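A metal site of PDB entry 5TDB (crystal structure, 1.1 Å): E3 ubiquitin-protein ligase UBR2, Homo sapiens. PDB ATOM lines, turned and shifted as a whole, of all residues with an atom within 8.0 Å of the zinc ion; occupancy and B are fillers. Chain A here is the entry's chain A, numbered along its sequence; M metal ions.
The backbone NH of His 41 is in hydrogen-bond range of the side-chain hydroxyl of Ser 39. The backbone carbonyl oxygen (O) of Cys 23 is in hydrogen-bond range of the backbone NH (N) of Lys 66, 2.8 Å away. NE2 of His 41 lies close to O of Glu 67, at 3.5 Å. The side-chain sulfur (SG) of Cys 20 sits close to the backbone NH (N) of Asp 22 (3.5 Å). NE2 of His 41 sits at hydrogen-bond distance from O of Gly 68, at 2.9 Å.
ND1 of His 44 is bound to the zinc ion (2.0 Å). ND1 of His 41 is bound to the zinc ion. SG of Cys 20 binds the zinc ion (2.3 Å). SG of Cys 23 is bound to the zinc ion (2.3 Å). The zinc ion has four donor atoms within binding distance.
Within 4 Å of the zinc ion: Cys 20, Cys 23, His 41 and His 44. Along chain A the residues within 4 Å of the zinc ion span positions 20 to 44.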
ATOM      1  N   SER A  19      29.382 -18.665  -6.666  1.00  0.00           N
ATOM      2  CA  SER A  19      28.845 -19.876  -6.064  1.00  0.00           C
ATOM      3  C   SER A  19      29.202 -19.829  -4.582  1.00  0.00           C
ATOM      4  O   SER A  19      30.004 -19.011  -4.133  1.00  0.00           O
ATOM      5  CB  SER A  19      29.368 -21.108  -6.786  1.00  0.00           C
ATOM      6  OG  SER A  19      28.690 -22.267  -6.368  1.00  0.00           O
ATOM      7  N   CYS A  20      28.511 -20.624  -3.793  1.00  0.00           N
ATOM      8  CA  CYS A  20      28.822 -20.777  -2.383  1.00  0.00           C
ATOM      9  C   CYS A  20      29.339 -22.186  -2.158  1.00  0.00           C
ATOM     10  O   CYS A  20      28.635 -23.152  -2.453  1.00  0.00           O
ATOM     11  CB  CYS A  20      27.592 -20.539  -1.518  1.00  0.00           C
ATOM     12  SG  CYS A  20      28.060 -20.654   0.237  1.00  0.00           S
ATOM     13  N   ARG A  21      30.574 -22.303  -1.664  1.00  0.00           N
ATOM     14  CA  ARG A  21      31.154 -23.620  -1.456  1.00  0.00           C
ATOM     15  C   ARG A  21      30.460 -24.353  -0.313  1.00  0.00           C
ATOM     16  O   ARG A  21      30.495 -25.580  -0.272  1.00  0.00           O
ATOM     17  CB  ARG A  21      32.663 -23.523  -1.209  1.00  0.00           C
ATOM     18  CG  ARG A  21      33.420 -23.012  -2.438  1.00  0.00           C
ATOM     19  CD  ARG A  21      34.796 -22.482  -2.082  1.00  0.00           C
ATOM     20  NE  ARG A  21      35.604 -23.529  -1.485  1.00  0.00           N
ATOM     21  CZ  ARG A  21      36.775 -23.331  -0.899  1.00  0.00           C
ATOM     22  NH1 ARG A  21      37.301 -22.114  -0.849  1.00  0.00           N
ATOM     23  NH2 ARG A  21      37.440 -24.367  -0.377  1.00  0.00           N
ATOM     24  N   ASP A  22      29.838 -23.618   0.603  1.00  0.00           N
ATOM     25  CA  ASP A  22      29.123 -24.241   1.710  1.00  0.00           C
ATOM     26  C   ASP A  22      27.717 -24.697   1.332  1.00  0.00           C
ATOM     27  O   ASP A  22      27.238 -25.695   1.890  1.00  0.00           O
ATOM     28  CB  ASP A  22      29.044 -23.269   2.884  1.00  0.00           C
ATOM     29  CG  ASP A  22      30.403 -22.881   3.424  1.00  0.00           C
ATOM     30  OD1 ASP A  22      31.230 -23.785   3.668  1.00  0.00           O
ATOM     31  OD2 ASP A  22      30.639 -21.676   3.649  1.00  0.00           O
ATOM     32  N   CYS A  23      27.023 -23.999   0.430  1.00  0.00           N
ATOM     33  CA  CYS A  23      25.603 -24.229   0.209  1.00  0.00           C
ATOM     34  C   CYS A  23      25.233 -24.737  -1.179  1.00  0.00           C
ATOM     35  O   CYS A  23      24.136 -25.289  -1.344  1.00  0.00           O
ATOM     36  CB  CYS A  23      24.768 -22.955   0.475  1.00  0.00           C
ATOM     37  SG  CYS A  23      25.047 -22.231   2.136  1.00  0.00           S
ATOM     38  N   ALA A  24      26.091 -24.573  -2.176  1.00  0.00           N
ATOM     39  CA  ALA A  24      25.722 -25.001  -3.523  1.00  0.00           C
ATOM     40  C   ALA A  24      25.513 -26.512  -3.552  1.00  0.00           C
ATOM     41  O   ALA A  24      26.280 -27.271  -2.955  1.00  0.00           O
ATOM     42  CB  ALA A  24      26.807 -24.615  -4.520  1.00  0.00           C
ATOM     43  N   LEU A  31      24.947 -17.557  -8.375  1.00  0.00           N
ATOM     44  CA  LEU A  31      24.187 -16.336  -8.209  1.00  0.00           C
ATOM     45  C   LEU A  31      24.826 -15.191  -8.988  1.00  0.00           C
ATOM     46  O   LEU A  31      26.059 -15.097  -9.091  1.00  0.00           O
ATOM     47  CB  LEU A  31      24.116 -15.938  -6.734  1.00  0.00           C
ATOM     48  CG  LEU A  31      23.392 -16.938  -5.830  1.00  0.00           C
ATOM     49  CD1 LEU A  31      23.506 -16.509  -4.391  1.00  0.00           C
ATOM     50  CD2 LEU A  31      21.937 -17.101  -6.211  1.00  0.00           C
ATOM     51  N   PHE A  36      23.825 -12.392  -5.096  1.00  0.00           N
ATOM     52  CA  PHE A  36      24.883 -12.754  -4.158  1.00  0.00           C
ATOM     53  C   PHE A  36      24.989 -11.724  -3.029  1.00  0.00           C
ATOM     54  O   PHE A  36      25.039 -12.091  -1.852  1.00  0.00           O
ATOM     55  CB  PHE A  36      26.226 -12.892  -4.911  1.00  0.00           C
ATOM     56  CG  PHE A  36      27.395 -13.029  -4.000  1.00  0.00           C
ATOM     57  CD1 PHE A  36      27.614 -14.201  -3.280  1.00  0.00           C
ATOM     58  CD2 PHE A  36      28.307 -11.982  -3.850  1.00  0.00           C
ATOM     59  CE1 PHE A  36      28.715 -14.312  -2.437  1.00  0.00           C
ATOM     60  CE2 PHE A  36      29.379 -12.099  -3.011  1.00  0.00           C
ATOM     61  CZ  PHE A  36      29.571 -13.263  -2.305  1.00  0.00           C
ATOM     62  N   SER A  39      22.326 -11.943  -0.348  1.00  0.00           N
ATOM     63  CA  SER A  39      22.087 -13.314   0.105  1.00  0.00           C
ATOM     64  C   SER A  39      22.916 -13.603   1.358  1.00  0.00           C
ATOM     65  O   SER A  39      23.855 -12.883   1.701  1.00  0.00           O
ATOM     66  CB  SER A  39      22.473 -14.334  -0.979  1.00  0.00           C
ATOM     67  OG  SER A  39      23.880 -14.529  -1.057  1.00  0.00           O
ATOM     68  N   ILE A  40      22.582 -14.711   2.028  1.00  0.00           N
ATOM     69  CA  ILE A  40      23.396 -15.153   3.161  1.00  0.00           C
ATOM     70  C   ILE A  40      24.798 -15.563   2.759  1.00  0.00           C
ATOM     71  O   ILE A  40      25.691 -15.607   3.611  1.00  0.00           O
ATOM     72  CB  ILE A  40      22.742 -16.316   3.942  1.00  0.00           C
ATOM     73  CG1 ILE A  40      22.635 -17.575   3.079  1.00  0.00           C
ATOM     74  CG2 ILE A  40      21.409 -15.915   4.493  1.00  0.00           C
ATOM     75  CD1 ILE A  40      22.299 -18.825   3.841  1.00  0.00           C
ATOM     76  N   HIS A  41      25.025 -15.893   1.483  1.00  0.00           N
ATOM     77  CA  HIS A  41      26.284 -16.500   1.048  1.00  0.00           C
ATOM     78  C   HIS A  41      27.429 -15.506   0.988  1.00  0.00           C
ATOM     79  O   HIS A  41      28.589 -15.932   0.933  1.00  0.00           O
ATOM     80  CB  HIS A  41      26.067 -17.199  -0.284  1.00  0.00           C
ATOM     81  CG  HIS A  41      24.862 -18.077  -0.282  1.00  0.00           C
ATOM     82  ND1 HIS A  41      24.785 -19.237   0.464  1.00  0.00           N
ATOM     83  CD2 HIS A  41      23.660 -17.921  -0.869  1.00  0.00           C
ATOM     84  CE1 HIS A  41      23.575 -19.762   0.298  1.00  0.00           C
ATOM     85  NE2 HIS A  41      22.871 -18.975  -0.502  1.00  0.00           N
ATOM     86  N   ARG A  42      27.154 -14.202   1.042  1.00  0.00           N
ATOM     87  CA  ARG A  42      28.254 -13.256   1.113  1.00  0.00           C
ATOM     88  C   ARG A  42      29.029 -13.389   2.417  1.00  0.00           C
ATOM     89  O   ARG A  42      30.140 -12.874   2.497  1.00  0.00           O
ATOM     90  CB  ARG A  42      27.749 -11.836   0.907  1.00  0.00           C
ATOM     91  CG  ARG A  42      26.889 -11.296   2.023  1.00  0.00           C
ATOM     92  CD  ARG A  42      26.552  -9.829   1.761  1.00  0.00           C
ATOM     93  NE  ARG A  42      27.742  -8.988   1.816  1.00  0.00           N
ATOM     94  CZ  ARG A  42      27.936  -7.859   1.141  1.00  0.00           C
ATOM     95  NH1 ARG A  42      27.013  -7.378   0.328  1.00  0.00           N
ATOM     96  NH2 ARG A  42      29.064  -7.208   1.284  1.00  0.00           N
ATOM     97  N   ASP A  43      28.494 -14.094   3.409  1.00  0.00           N
ATOM     98  CA  ASP A  43      29.175 -14.385   4.663  1.00  0.00           C
ATOM     99  C   ASP A  43      29.750 -15.803   4.725  1.00  0.00           C
ATOM    100  O   ASP A  43      30.212 -16.226   5.786  1.00  0.00           O
ATOM    101  CB  ASP A  43      28.205 -14.184   5.821  1.00  0.00           C
ATOM    102  CG  ASP A  43      27.832 -12.737   6.025  1.00  0.00           C
ATOM    103  OD1 ASP A  43      28.716 -11.865   5.876  1.00  0.00           O
ATOM    104  OD2 ASP A  43      26.665 -12.462   6.337  1.00  0.00           O
ATOM    105  N   HIS A  44      29.753 -16.521   3.598  1.00  0.00           N
ATOM    106  CA  HIS A  44      30.193 -17.908   3.489  1.00  0.00           C
ATOM    107  C   HIS A  44      31.467 -17.999   2.646  1.00  0.00           C
ATOM    108  O   HIS A  44      32.010 -16.991   2.192  1.00  0.00           O
ATOM    109  CB  HIS A  44      29.073 -18.754   2.882  1.00  0.00           C
ATOM    110  CG  HIS A  44      27.838 -18.829   3.721  1.00  0.00           C
ATOM    111  ND1 HIS A  44      26.663 -19.406   3.286  1.00  0.00           N
ATOM    112  CD2 HIS A  44      27.593 -18.387   4.984  1.00  0.00           C
ATOM    113  CE1 HIS A  44      25.769 -19.348   4.258  1.00  0.00           C
ATOM    114  NE2 HIS A  44      26.295 -18.725   5.295  1.00  0.00           N
ATOM    115  N   ARG A  45      31.960 -19.232   2.464  1.00  0.00           N
ATOM    116  CA  ARG A  45      33.092 -19.485   1.557  1.00  0.00           C
ATOM    117  C   ARG A  45      32.576 -19.483   0.120  1.00  0.00           C
ATOM    118  O   ARG A  45      32.105 -20.494  -0.373  1.00  0.00           O
ATOM    119  CB  ARG A  45      33.709 -20.842   1.850  1.00  0.00           C
ATOM    120  CG  ARG A  45      34.508 -20.950   3.112  1.00  0.00           C
ATOM    121  CD  ARG A  45      35.164 -22.321   3.186  1.00  0.00           C
ATOM    122  NE  ARG A  45      34.168 -23.373   2.980  1.00  0.00           N
ATOM    123  CZ  ARG A  45      34.405 -24.531   2.363  1.00  0.00           C
ATOM    124  NH1 ARG A  45      35.604 -24.826   1.896  1.00  0.00           N
ATOM    125  NH2 ARG A  45      33.407 -25.394   2.204  1.00  0.00           N
ATOM    126  N   TYR A  46      32.699 -18.362  -0.560  1.00  0.00           N
ATOM    127  CA  TYR A  46      32.175 -18.265  -1.916  1.00  0.00           C
ATOM    128  C   TYR A  46      33.292 -18.352  -2.954  1.00  0.00           C
ATOM    129  O   TYR A  46      34.486 -18.209  -2.643  1.00  0.00           O
ATOM    130  CB  TYR A  46      31.388 -16.961  -2.098  1.00  0.00           C
ATOM    131  CG  TYR A  46      32.201 -15.714  -1.849  1.00  0.00           C
ATOM    132  CD1 TYR A  46      32.943 -15.133  -2.854  1.00  0.00           C
ATOM    133  CD2 TYR A  46      32.209 -15.119  -0.601  1.00  0.00           C
ATOM    134  CE1 TYR A  46      33.679 -13.990  -2.631  1.00  0.00           C
ATOM    135  CE2 TYR A  46      32.943 -13.983  -0.357  1.00  0.00           C
ATOM    136  CZ  TYR A  46      33.668 -13.413  -1.371  1.00  0.00           C
ATOM    137  OH  TYR A  46      34.402 -12.277  -1.127  1.00  0.00           O
ATOM    138  N   TRP A  65      20.341 -25.028  -3.787  1.00  0.00           N
ATOM    139  CA  TRP A  65      20.979 -24.520  -2.576  1.00  0.00           C
ATOM    140  C   TRP A  65      20.542 -25.334  -1.371  1.00  0.00           C
ATOM    141  O   TRP A  65      19.340 -25.584  -1.184  1.00  0.00           O
ATOM    142  CB  TRP A  65      20.621 -23.034  -2.371  1.00  0.00           C
ATOM    143  CG  TRP A  65      20.924 -22.204  -3.577  1.00  0.00           C
ATOM    144  CD1 TRP A  65      20.026 -21.751  -4.514  1.00  0.00           C
ATOM    145  CD2 TRP A  65      22.223 -21.806  -4.019  1.00  0.00           C
ATOM    146  NE1 TRP A  65      20.693 -21.069  -5.483  1.00  0.00           N
ATOM    147  CE2 TRP A  65      22.037 -21.077  -5.218  1.00  0.00           C
ATOM    148  CE3 TRP A  65      23.520 -21.960  -3.518  1.00  0.00           C
ATOM    149  CZ2 TRP A  65      23.090 -20.551  -5.927  1.00  0.00           C
ATOM    150  CZ3 TRP A  65      24.564 -21.435  -4.209  1.00  0.00           C
ATOM    151  CH2 TRP A  65      24.347 -20.727  -5.403  1.00  0.00           C
ATOM    152  N   LYS A  66      21.506 -25.704  -0.529  1.00  0.00           N
ATOM    153  CA  LYS A  66      21.190 -26.435   0.690  1.00  0.00           C
ATOM    154  C   LYS A  66      20.599 -25.530   1.748  1.00  0.00           C
ATOM    155  O   LYS A  66      19.877 -25.996   2.636  1.00  0.00           O
ATOM    156  CB  LYS A  66      22.442 -27.140   1.217  1.00  0.00           C
ATOM    157  CG  LYS A  66      22.856 -28.278   0.309  1.00  0.00           C
ATOM    158  CD  LYS A  66      24.037 -29.048   0.829  1.00  0.00           C
ATOM    159  CE  LYS A  66      25.311 -28.271   0.606  1.00  0.00           C
ATOM    160  NZ  LYS A  66      26.503 -29.164   0.657  1.00  0.00           N
ATOM    161  N   GLU A  67      20.869 -24.235   1.646  1.00  0.00           N
ATOM    162  CA  GLU A  67      20.373 -23.201   2.537  1.00  0.00           C
ATOM    163  C   GLU A  67      20.378 -21.898   1.742  1.00  0.00           C
ATOM    164  O   GLU A  67      21.159 -21.726   0.806  1.00  0.00           O
ATOM    165  CB  GLU A  67      21.322 -23.092   3.735  1.00  0.00           C
ATOM    166  CG  GLU A  67      21.014 -21.994   4.719  1.00  0.00           C
ATOM    167  CD  GLU A  67      21.929 -22.036   5.923  1.00  0.00           C
ATOM    168  OE1 GLU A  67      22.780 -22.955   6.008  1.00  0.00           O
ATOM    169  OE2 GLU A  67      21.811 -21.149   6.798  1.00  0.00           O
ATOM    170  N   GLY A  68      19.489 -20.986   2.122  1.00  0.00           N
ATOM    171  CA  GLY A  68      19.486 -19.641   1.552  1.00  0.00           C
ATOM    172  C   GLY A  68      19.260 -19.560   0.046  1.00  0.00           C
ATOM    173  O   GLY A  68      20.003 -18.890  -0.680  1.00  0.00           O
HETATM  174 ZN    ZN M   1      26.201 -20.344   1.536  1.00  0.00          ZN
